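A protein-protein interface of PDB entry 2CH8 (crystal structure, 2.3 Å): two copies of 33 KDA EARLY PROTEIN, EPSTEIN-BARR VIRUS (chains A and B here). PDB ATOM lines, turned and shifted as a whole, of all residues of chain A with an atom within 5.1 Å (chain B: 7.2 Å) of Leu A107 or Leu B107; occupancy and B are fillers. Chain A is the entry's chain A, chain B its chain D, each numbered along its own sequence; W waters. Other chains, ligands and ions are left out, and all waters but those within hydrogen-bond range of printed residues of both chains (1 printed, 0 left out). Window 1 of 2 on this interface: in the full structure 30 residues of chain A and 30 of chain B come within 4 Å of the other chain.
Of the printed residues of chain A, His B110 touches Leu A105 and Thr A106. Of the printed residues of chain A, Val B109 touches Leu A105, Thr A106, Leu A107 and Ala A190. Of the printed residues of chain B, Ser A108 touches Leu B107 (3.2 Å) and Ser B108 (3.1 Å). Of the printed residues of chain B, Gly A192 touches His B191. The nearest printed residue of chain B that does not touch Leu A107 is His B110 (5.2 Å).
Leu A105 touches Val B109, and with the chains exchanged Val A109 touches Leu B105. Thr A106 touches Val B109, and with the chains exchanged Val A109 touches Thr B106. Leu A107 touches Ser B108, and with the chains exchanged Ser A108 touches Leu B107. His A191 touches Gly B192, and with the chains exchanged Gly A192 touches His B191. 14 positions are printed for both chains. Of the 17 pairs that touch across the chains among the printed residues, 12 have their exchanged pair printed and touching as well.
N of Val B109 lies within hydrogen-bond range of O of Leu A107, at 2.8 Å. The backbone NH (N) of Val A109 lies within hydrogen-bond range of the backbone carbonyl oxygen (O) of Leu B107, at 2.9 Å. The backbone NH of His A191 sits at hydrogen-bond distance from the backbone carbonyl oxygen of Val B193. OG of Ser A108 sits at hydrogen-bond distance from OG of Ser B108 (3.1 Å).
Hydrophobic or aromatic side chains of chain A that line the printed part of chain B: Leu A107, Val A109 and Ala A190. Of the 23 printed residues of chain B, 9 touch a printed residue of chain A. Printed residues of chain B that touch a printed residue of chain A: Leu B105, Thr B106, Leu B107, Ser B108, Val B109, His B110, His B191, Gly B192 and Val B193. Along chain B the printed residues that touch a printed residue of chain A span positions 105 to 193. Among the printed residues, no Asp or Glu carboxylate lies within 4 Å of a Lys or Arg side-chain nitrogen of the other chain.
The backbone carbonyl oxygen (O) of His B110 lies within hydrogen-bond range of the backbone NH (N) of Thr B125. N of Ser A108 is in hydrogen-bond range of O of Thr A127 (2.8 Å). The side-chain sulfur (SG) of Cys B181 forms a disulfide with the side-chain sulfur (SG) of Cys B126 (2.0 Å). The backbone NH (N) of Ser B108 is in hydrogen-bond range of the backbone carbonyl oxygen (O) of Thr B127, 2.8 Å away. SG of Cys A126 forms a disulfide with SG of Cys A181 (2.0 Å). The backbone carbonyl oxygen of Asn B129 sits at hydrogen-bond distance from the backbone NH of Thr B106, at 2.7 Å.
Among the printed residues, pairs that only touch across the chains: Leu A105 with Val B109, Leu A105 with His B110, Thr A106 with Val B109, Thr A106 with His B110, Leu A107 with Leu B107, Leu A107 with Ser B108, Ser A108 with Leu B107, Val A109 with Leu B105, Val A109 with Thr B106, Ala A190 with Val B109, Ala A190 with Val B193, His A191 with Gly B192 and Gly A192 with His B191.
Water W1 bridges OG1 of Thr A106 and ND1 of His B110.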
ATOM      1  N   LEU A 105     -11.229   7.536  28.331  1.00  0.00           N
ATOM      2  CA  LEU A 105     -12.390   8.374  28.127  1.00  0.00           C
ATOM      3  C   LEU A 105     -13.636   7.532  27.959  1.00  0.00           C
ATOM      4  O   LEU A 105     -13.561   6.399  27.475  1.00  0.00           O
ATOM      5  CB  LEU A 105     -12.199   9.332  26.944  1.00  0.00           C
ATOM      6  CG  LEU A 105     -12.129   8.773  25.519  1.00  0.00           C
ATOM      7  CD1 LEU A 105     -13.455   8.330  24.992  1.00  0.00           C
ATOM      8  CD2 LEU A 105     -11.513   9.817  24.637  1.00  0.00           C
ATOM      9  N   THR A 106     -14.770   8.066  28.451  1.00  0.00           N
ATOM     10  CA  THR A 106     -16.101   7.566  28.097  1.00  0.00           C
ATOM     11  C   THR A 106     -16.768   8.656  27.222  1.00  0.00           C
ATOM     12  O   THR A 106     -16.876   9.809  27.635  1.00  0.00           O
ATOM     13  CB  THR A 106     -16.937   7.286  29.347  1.00  0.00           C
ATOM     14  OG1 THR A 106     -16.249   6.304  30.145  1.00  0.00           O
ATOM     15  CG2 THR A 106     -18.314   6.768  28.976  1.00  0.00           C
ATOM     16  N   LEU A 107     -17.165   8.300  26.008  1.00  0.00           N
ATOM     17  CA  LEU A 107     -17.934   9.230  25.178  1.00  0.00           C
ATOM     18  C   LEU A 107     -19.366   8.748  25.181  1.00  0.00           C
ATOM     19  O   LEU A 107     -19.605   7.574  24.850  1.00  0.00           O
ATOM     20  CB  LEU A 107     -17.357   9.326  23.744  1.00  0.00           C
ATOM     21  CG  LEU A 107     -17.945  10.362  22.736  1.00  0.00           C
ATOM     22  CD1 LEU A 107     -16.952  10.923  21.752  1.00  0.00           C
ATOM     23  CD2 LEU A 107     -19.188   9.845  21.992  1.00  0.00           C
ATOM     24  N   SER A 108     -20.295   9.643  25.577  1.00  0.00           N
ATOM     25  CA  SER A 108     -21.776   9.473  25.418  1.00  0.00           C
ATOM     26  C   SER A 108     -22.462  10.461  24.467  1.00  0.00           C
ATOM     27  O   SER A 108     -22.183  11.670  24.547  1.00  0.00           O
ATOM     28  CB  SER A 108     -22.453   9.648  26.755  1.00  0.00           C
ATOM     29  OG  SER A 108     -21.831   8.796  27.657  1.00  0.00           O
ATOM     30  N   VAL A 109     -23.358   9.940  23.604  1.00  0.00           N
ATOM     31  CA  VAL A 109     -24.314  10.727  22.816  1.00  0.00           C
ATOM     32  C   VAL A 109     -25.771  10.391  23.143  1.00  0.00           C
ATOM     33  O   VAL A 109     -26.138   9.225  23.295  1.00  0.00           O
ATOM     34  CB  VAL A 109     -24.239  10.546  21.239  1.00  0.00           C
ATOM     35  CG1 VAL A 109     -23.522  11.721  20.551  1.00  0.00           C
ATOM     36  CG2 VAL A 109     -23.728   9.192  20.811  1.00  0.00           C
ATOM     37  N   CYS A 126     -23.290  15.659  23.781  1.00  0.00           N
ATOM     38  CA  CYS A 126     -22.139  14.793  23.742  1.00  0.00           C
ATOM     39  C   CYS A 126     -21.292  15.043  24.950  1.00  0.00           C
ATOM     40  O   CYS A 126     -20.929  16.181  25.222  1.00  0.00           O
ATOM     41  CB  CYS A 126     -21.318  15.073  22.525  1.00  0.00           C
ATOM     42  SG  CYS A 126     -19.962  13.861  22.396  1.00  0.00           S
ATOM     43  N   THR A 127     -20.972  13.974  25.671  1.00  0.00           N
ATOM     44  CA  THR A 127     -20.338  14.091  26.989  1.00  0.00           C
ATOM     45  C   THR A 127     -19.113  13.217  26.900  1.00  0.00           C
ATOM     46  O   THR A 127     -19.192  12.048  26.407  1.00  0.00           O
ATOM     47  CB  THR A 127     -21.258  13.545  28.125  1.00  0.00           C
ATOM     48  OG1 THR A 127     -22.496  14.295  28.178  1.00  0.00           O
ATOM     49  CG2 THR A 127     -20.593  13.647  29.462  1.00  0.00           C
ATOM     50  N   VAL A 128     -17.971  13.795  27.302  1.00  0.00           N
ATOM     51  CA  VAL A 128     -16.700  13.031  27.500  1.00  0.00           C
ATOM     52  C   VAL A 128     -16.236  13.099  28.975  1.00  0.00           C
ATOM     53  O   VAL A 128     -16.060  14.204  29.532  1.00  0.00           O
ATOM     54  CB  VAL A 128     -15.599  13.479  26.529  1.00  0.00           C
ATOM     55  CG1 VAL A 128     -14.299  12.753  26.797  1.00  0.00           C
ATOM     56  CG2 VAL A 128     -16.031  13.179  25.118  1.00  0.00           C
ATOM     57  N   CYS A 181     -19.800  13.858  16.894  1.00  0.00           N
ATOM     58  CA  CYS A 181     -19.143  14.283  18.115  1.00  0.00           C
ATOM     59  C   CYS A 181     -17.665  13.741  18.148  1.00  0.00           C
ATOM     60  O   CYS A 181     -17.437  12.555  17.957  1.00  0.00           O
ATOM     61  CB  CYS A 181     -19.963  13.731  19.330  1.00  0.00           C
ATOM     62  SG  CYS A 181     -19.169  14.409  20.647  1.00  0.00           S
ATOM     63  N   VAL A 182     -16.671  14.592  18.343  1.00  0.00           N
ATOM     64  CA  VAL A 182     -15.284  14.115  18.502  1.00  0.00           C
ATOM     65  C   VAL A 182     -14.804  14.220  19.984  1.00  0.00           C
ATOM     66  O   VAL A 182     -14.731  15.331  20.556  1.00  0.00           O
ATOM     67  CB  VAL A 182     -14.272  14.876  17.587  1.00  0.00           C
ATOM     68  CG1 VAL A 182     -12.842  14.382  17.849  1.00  0.00           C
ATOM     69  CG2 VAL A 182     -14.593  14.708  16.088  1.00  0.00           C
ATOM     70  N   GLY A 183     -14.478  13.086  20.602  1.00  0.00           N
ATOM     71  CA  GLY A 183     -13.952  13.100  21.998  1.00  0.00           C
ATOM     72  C   GLY A 183     -12.472  12.754  22.092  1.00  0.00           C
ATOM     73  O   GLY A 183     -12.000  11.874  21.396  1.00  0.00           O
ATOM     74  N   ALA A 190     -12.213   9.085  20.404  1.00  0.00           N
ATOM     75  CA  ALA A 190     -13.465   8.420  20.052  1.00  0.00           C
ATOM     76  C   ALA A 190     -14.505   9.373  19.367  1.00  0.00           C
ATOM     77  O   ALA A 190     -14.472  10.587  19.570  1.00  0.00           O
ATOM     78  CB  ALA A 190     -14.073   7.712  21.313  1.00  0.00           C
ATOM     79  N   HIS A 191     -15.426   8.826  18.572  1.00  0.00           N
ATOM     80  CA  HIS A 191     -16.512   9.660  18.001  1.00  0.00           C
ATOM     81  C   HIS A 191     -17.844   9.070  18.367  1.00  0.00           C
ATOM     82  O   HIS A 191     -17.966   7.871  18.600  1.00  0.00           O
ATOM     83  CB  HIS A 191     -16.515   9.746  16.458  1.00  0.00           C
ATOM     84  CG  HIS A 191     -15.226  10.191  15.844  1.00  0.00           C
ATOM     85  ND1 HIS A 191     -14.924   9.946  14.524  1.00  0.00           N
ATOM     86  CD2 HIS A 191     -14.156  10.837  16.362  1.00  0.00           C
ATOM     87  CE1 HIS A 191     -13.725  10.423  14.250  1.00  0.00           C
ATOM     88  NE2 HIS A 191     -13.234  10.962  15.353  1.00  0.00           N
ATOM     89  N   GLY A 192     -18.857   9.914  18.374  1.00  0.00           N
ATOM     90  CA  GLY A 192     -20.219   9.449  18.471  1.00  0.00           C
ATOM     91  C   GLY A 192     -20.988  10.209  17.411  1.00  0.00           C
ATOM     92  O   GLY A 192     -20.845  11.432  17.279  1.00  0.00           O
ATOM     93  N   PRO B 104     -35.194   8.430  24.520  1.00  0.00           N
ATOM     94  CA  PRO B 104     -34.168   8.508  23.458  1.00  0.00           C
ATOM     95  C   PRO B 104     -32.913   7.708  23.924  1.00  0.00           C
ATOM     96  O   PRO B 104     -32.620   7.680  25.119  1.00  0.00           O
ATOM     97  CB  PRO B 104     -33.834  10.001  23.387  1.00  0.00           C
ATOM     98  CG  PRO B 104     -34.959  10.696  24.062  1.00  0.00           C
ATOM     99  CD  PRO B 104     -35.588   9.751  25.044  1.00  0.00           C
ATOM    100  N   LEU B 105     -32.211   7.062  22.994  1.00  0.00           N
ATOM    101  CA  LEU B 105     -31.062   6.237  23.355  1.00  0.00           C
ATOM    102  C   LEU B 105     -29.859   7.062  23.824  1.00  0.00           C
ATOM    103  O   LEU B 105     -29.683   8.254  23.410  1.00  0.00           O
ATOM    104  CB  LEU B 105     -30.704   5.257  22.227  1.00  0.00           C
ATOM    105  CG  LEU B 105     -30.116   5.740  20.890  1.00  0.00           C
ATOM    106  CD1 LEU B 105     -28.655   6.313  21.012  1.00  0.00           C
ATOM    107  CD2 LEU B 105     -30.214   4.604  19.887  1.00  0.00           C
ATOM    108  N   THR B 106     -29.102   6.492  24.765  1.00  0.00           N
ATOM    109  CA  THR B 106     -27.770   6.986  25.066  1.00  0.00           C
ATOM    110  C   THR B 106     -26.765   5.900  24.644  1.00  0.00           C
ATOM    111  O   THR B 106     -26.841   4.773  25.116  1.00  0.00           O
ATOM    112  CB  THR B 106     -27.626   7.354  26.568  1.00  0.00           C
ATOM    113  OG1 THR B 106     -28.664   8.276  26.950  1.00  0.00           O
ATOM    114  CG2 THR B 106     -26.208   7.938  26.931  1.00  0.00           C
ATOM    115  N   LEU B 107     -25.874   6.240  23.720  1.00  0.00           N
ATOM    116  CA  LEU B 107     -24.755   5.381  23.264  1.00  0.00           C
ATOM    117  C   LEU B 107     -23.509   5.837  23.990  1.00  0.00           C
ATOM    118  O   LEU B 107     -23.126   7.015  23.851  1.00  0.00           O
ATOM    119  CB  LEU B 107     -24.520   5.482  21.734  1.00  0.00           C
ATOM    120  CG  LEU B 107     -23.537   4.435  21.106  1.00  0.00           C
ATOM    121  CD1 LEU B 107     -23.950   3.988  19.715  1.00  0.00           C
ATOM    122  CD2 LEU B 107     -22.089   4.921  21.087  1.00  0.00           C
ATOM    123  N   SER B 108     -22.897   4.951  24.779  1.00  0.00           N
ATOM    124  CA  SER B 108     -21.541   5.186  25.359  1.00  0.00           C
ATOM    125  C   SER B 108     -20.490   4.240  24.807  1.00  0.00           C
ATOM    126  O   SER B 108     -20.735   3.017  24.701  1.00  0.00           O
ATOM    127  CB  SER B 108     -21.515   4.994  26.890  1.00  0.00           C
ATOM    128  OG  SER B 108     -22.460   5.792  27.508  1.00  0.00           O
ATOM    129  N   VAL B 109     -19.321   4.799  24.490  1.00  0.00           N
ATOM    130  CA  VAL B 109     -18.106   3.986  24.186  1.00  0.00           C
ATOM    131  C   VAL B 109     -16.986   4.256  25.198  1.00  0.00           C
ATOM    132  O   VAL B 109     -16.752   5.408  25.584  1.00  0.00           O
ATOM    133  CB  VAL B 109     -17.571   4.154  22.735  1.00  0.00           C
ATOM    134  CG1 VAL B 109     -18.566   3.723  21.785  1.00  0.00           C
ATOM    135  CG2 VAL B 109     -17.195   5.612  22.396  1.00  0.00           C
ATOM    136  N   HIS B 110     -16.343   3.172  25.646  1.00  0.00           N
ATOM    137  CA  HIS B 110     -15.182   3.210  26.534  1.00  0.00           C
ATOM    138  C   HIS B 110     -14.286   1.936  26.292  1.00  0.00           C
ATOM    139  O   HIS B 110     -14.754   0.877  25.858  1.00  0.00           O
ATOM    140  CB  HIS B 110     -15.670   3.496  27.981  1.00  0.00           C
ATOM    141  CG  HIS B 110     -15.948   2.294  28.819  1.00  0.00           C
ATOM    142  ND1 HIS B 110     -17.211   1.748  28.940  1.00  0.00           N
ATOM    143  CD2 HIS B 110     -15.147   1.583  29.654  1.00  0.00           C
ATOM    144  CE1 HIS B 110     -17.163   0.714  29.767  1.00  0.00           C
ATOM    145  NE2 HIS B 110     -15.921   0.590  30.209  1.00  0.00           N
ATOM    146  N   THR B 125     -15.955  -1.445  24.985  1.00  0.00           N
ATOM    147  CA  THR B 125     -17.334  -1.604  25.438  1.00  0.00           C
ATOM    148  C   THR B 125     -18.268  -0.545  24.868  1.00  0.00           C
ATOM    149  O   THR B 125     -17.971   0.659  24.846  1.00  0.00           O
ATOM    150  CB  THR B 125     -17.404  -1.597  26.935  1.00  0.00           C
ATOM    151  OG1 THR B 125     -16.542  -2.625  27.387  1.00  0.00           O
ATOM    152  CG2 THR B 125     -18.867  -1.833  27.475  1.00  0.00           C
ATOM    153  N   CYS B 126     -19.374  -1.031  24.344  1.00  0.00           N
ATOM    154  CA  CYS B 126     -20.382  -0.174  23.784  1.00  0.00           C
ATOM    155  C   CYS B 126     -21.710  -0.454  24.472  1.00  0.00           C
ATOM    156  O   CYS B 126     -22.183  -1.571  24.459  1.00  0.00           O
ATOM    157  CB  CYS B 126     -20.509  -0.350  22.276  1.00  0.00           C
ATOM    158  SG  CYS B 126     -21.659   0.930  21.602  1.00  0.00           S
ATOM    159  N   THR B 127     -22.284   0.593  25.037  1.00  0.00           N
ATOM    160  CA  THR B 127     -23.505   0.552  25.875  1.00  0.00           C
ATOM    161  C   THR B 127     -24.618   1.412  25.252  1.00  0.00           C
ATOM    162  O   THR B 127     -24.399   2.554  24.881  1.00  0.00           O
ATOM    163  CB  THR B 127     -23.215   1.112  27.267  1.00  0.00           C
ATOM    164  OG1 THR B 127     -22.010   0.512  27.780  1.00  0.00           O
ATOM    165  CG2 THR B 127     -24.359   0.837  28.256  1.00  0.00           C
ATOM    166  N   VAL B 128     -25.800   0.837  25.112  1.00  0.00           N
ATOM    167  CA  VAL B 128     -26.977   1.607  24.672  1.00  0.00           C
ATOM    168  C   VAL B 128     -27.994   1.536  25.793  1.00  0.00           C
ATOM    169  O   VAL B 128     -28.393   0.459  26.198  1.00  0.00           O
ATOM    170  CB  VAL B 128     -27.548   1.136  23.319  1.00  0.00           C
ATOM    171  CG1 VAL B 128     -28.912   1.782  23.002  1.00  0.00           C
ATOM    172  CG2 VAL B 128     -26.558   1.439  22.199  1.00  0.00           C
ATOM    173  N   ASN B 129     -28.356   2.682  26.344  1.00  0.00           N
ATOM    174  CA  ASN B 129     -29.543   2.735  27.183  1.00  0.00           C
ATOM    175  C   ASN B 129     -30.715   3.359  26.401  1.00  0.00           C
ATOM    176  O   ASN B 129     -30.555   4.391  25.755  1.00  0.00           O
ATOM    177  CB  ASN B 129     -29.252   3.559  28.447  1.00  0.00           C
ATOM    178  CG  ASN B 129     -30.517   3.926  29.202  1.00  0.00           C
ATOM    179  OD1 ASN B 129     -31.109   4.977  28.973  1.00  0.00           O
ATOM    180  ND2 ASN B 129     -30.937   3.055  30.090  1.00  0.00           N
ATOM    181  N   HIS B 135     -30.446  -1.658  21.279  1.00  0.00           N
ATOM    182  CA  HIS B 135     -29.792  -2.731  20.546  1.00  0.00           C
ATOM    183  C   HIS B 135     -28.381  -2.234  20.274  1.00  0.00           C
ATOM    184  O   HIS B 135     -28.170  -1.045  20.041  1.00  0.00           O
ATOM    185  CB  HIS B 135     -30.593  -3.085  19.268  1.00  0.00           C
ATOM    186  CG  HIS B 135     -29.955  -4.133  18.422  1.00  0.00           C
ATOM    187  ND1 HIS B 135     -28.955  -3.850  17.510  1.00  0.00           N
ATOM    188  CD2 HIS B 135     -30.154  -5.474  18.364  1.00  0.00           C
ATOM    189  CE1 HIS B 135     -28.572  -4.974  16.930  1.00  0.00           C
ATOM    190  NE2 HIS B 135     -29.272  -5.972  17.440  1.00  0.00           N
ATOM    191  N   VAL B 136     -27.415  -3.145  20.356  1.00  0.00           N
ATOM    192  CA  VAL B 136     -25.989  -2.826  20.163  1.00  0.00           C
ATOM    193  C   VAL B 136     -25.323  -3.839  19.224  1.00  0.00           C
ATOM    194  O   VAL B 136     -25.546  -5.038  19.350  1.00  0.00           O
ATOM    195  CB  VAL B 136     -25.187  -2.866  21.509  1.00  0.00           C
ATOM    196  CG1 VAL B 136     -23.750  -2.420  21.265  1.00  0.00           C
ATOM    197  CG2 VAL B 136     -25.765  -1.954  22.473  1.00  0.00           C
ATOM    198  N   CYS B 181     -19.381   1.058  16.636  1.00  0.00           N
ATOM    199  CA  CYS B 181     -20.499   0.519  17.387  1.00  0.00           C
ATOM    200  C   CYS B 181     -21.824   1.076  16.812  1.00  0.00           C
ATOM    201  O   CYS B 181     -21.954   2.292  16.720  1.00  0.00           O
ATOM    202  CB  CYS B 181     -20.361   0.977  18.870  1.00  0.00           C
ATOM    203  SG  CYS B 181     -21.763   0.350  19.720  1.00  0.00           S
ATOM    204  N   VAL B 182     -22.789   0.227  16.434  1.00  0.00           N
ATOM    205  CA  VAL B 182     -24.120   0.727  15.975  1.00  0.00           C
ATOM    206  C   VAL B 182     -25.204   0.578  17.052  1.00  0.00           C
ATOM    207  O   VAL B 182     -25.546  -0.537  17.422  1.00  0.00           O
ATOM    208  CB  VAL B 182     -24.636   0.029  14.661  1.00  0.00           C
ATOM    209  CG1 VAL B 182     -26.000   0.570  14.278  1.00  0.00           C
ATOM    210  CG2 VAL B 182     -23.661   0.221  13.484  1.00  0.00           C
ATOM    211  N   GLY B 183     -25.726   1.701  17.552  1.00  0.00           N
ATOM    212  CA  GLY B 183     -26.798   1.705  18.546  1.00  0.00           C
ATOM    213  C   GLY B 183     -28.133   1.997  17.883  1.00  0.00           C
ATOM    214  O   GLY B 183     -28.212   2.812  16.979  1.00  0.00           O
ATOM    215  N   LYS B 184     -29.173   1.280  18.281  1.00  0.00           N
ATOM    216  CA  LYS B 184     -30.455   1.456  17.686  1.00  0.00           C
ATOM    217  C   LYS B 184     -31.529   1.507  18.777  1.00  0.00           C
ATOM    218  O   LYS B 184     -31.357   0.954  19.860  1.00  0.00           O
ATOM    219  CB  LYS B 184     -30.699   0.358  16.640  1.00  0.00           C
ATOM    220  CG  LYS B 184     -29.965   0.680  15.345  1.00  0.00           C
ATOM    221  CD  LYS B 184     -30.392  -0.169  14.254  1.00  0.00           C
ATOM    222  CE  LYS B 184     -30.661   0.689  13.002  1.00  0.00           C
ATOM    223  NZ  LYS B 184     -31.760   1.747  13.219  1.00  0.00           N
ATOM    224  N   GLU B 189     -30.871   5.798  15.714  1.00  0.00           N
ATOM    225  CA  GLU B 189     -29.570   5.150  15.509  1.00  0.00           C
ATOM    226  C   GLU B 189     -28.468   6.116  15.853  1.00  0.00           C
ATOM    227  O   GLU B 189     -28.519   7.281  15.497  1.00  0.00           O
ATOM    228  CB  GLU B 189     -29.458   4.643  14.051  1.00  0.00           C
ATOM    229  CG  GLU B 189     -28.093   4.159  13.647  1.00  0.00           C
ATOM    230  CD  GLU B 189     -28.025   3.474  12.267  1.00  0.00           C
ATOM    231  OE1 GLU B 189     -26.889   3.130  11.851  1.00  0.00           O
ATOM    232  OE2 GLU B 189     -29.083   3.277  11.603  1.00  0.00           O
ATOM    233  N   ALA B 190     -27.474   5.643  16.591  1.00  0.00           N
ATOM    234  CA  ALA B 190     -26.232   6.389  16.716  1.00  0.00           C
ATOM    235  C   ALA B 190     -25.068   5.419  16.498  1.00  0.00           C
ATOM    236  O   ALA B 190     -25.239   4.196  16.582  1.00  0.00           O
ATOM    237  CB  ALA B 190     -26.141   7.061  18.074  1.00  0.00           C
ATOM    238  N   HIS B 191     -23.895   5.975  16.228  1.00  0.00           N
ATOM    239  CA  HIS B 191     -22.666   5.210  16.116  1.00  0.00           C
ATOM    240  C   HIS B 191     -21.702   5.666  17.185  1.00  0.00           C
ATOM    241  O   HIS B 191     -21.727   6.827  17.582  1.00  0.00           O
ATOM    242  CB  HIS B 191     -22.030   5.419  14.736  1.00  0.00           C
ATOM    243  CG  HIS B 191     -22.836   4.844  13.616  1.00  0.00           C
ATOM    244  ND1 HIS B 191     -22.504   5.023  12.292  1.00  0.00           N
ATOM    245  CD2 HIS B 191     -23.944   4.067  13.626  1.00  0.00           C
ATOM    246  CE1 HIS B 191     -23.375   4.380  11.532  1.00  0.00           C
ATOM    247  NE2 HIS B 191     -24.254   3.785  12.318  1.00  0.00           N
ATOM    248  N   GLY B 192     -20.868   4.745  17.651  1.00  0.00           N
ATOM    249  CA  GLY B 192     -19.756   5.084  18.523  1.00  0.00           C
ATOM    250  C   GLY B 192     -18.530   4.509  17.845  1.00  0.00           C
ATOM    251  O   GLY B 192     -18.546   3.338  17.436  1.00  0.00           O
ATOM    252  N   VAL B 193     -17.508   5.351  17.656  1.00  0.00           N
ATOM    253  CA  VAL B 193     -16.260   4.961  16.956  1.00  0.00           C
ATOM    254  C   VAL B 193     -15.063   5.156  17.895  1.00  0.00           C
ATOM    255  O   VAL B 193     -14.789   6.296  18.318  1.00  0.00           O
ATOM    256  CB  VAL B 193     -16.052   5.793  15.649  1.00  0.00           C
ATOM    257  CG1 VAL B 193     -14.935   5.227  14.805  1.00  0.00           C
ATOM    258  CG2 VAL B 193     -17.303   5.821  14.845  1.00  0.00           C
HETATM  259  O   HOH W   1     -17.284   4.148  31.177  1.00  0.00           O
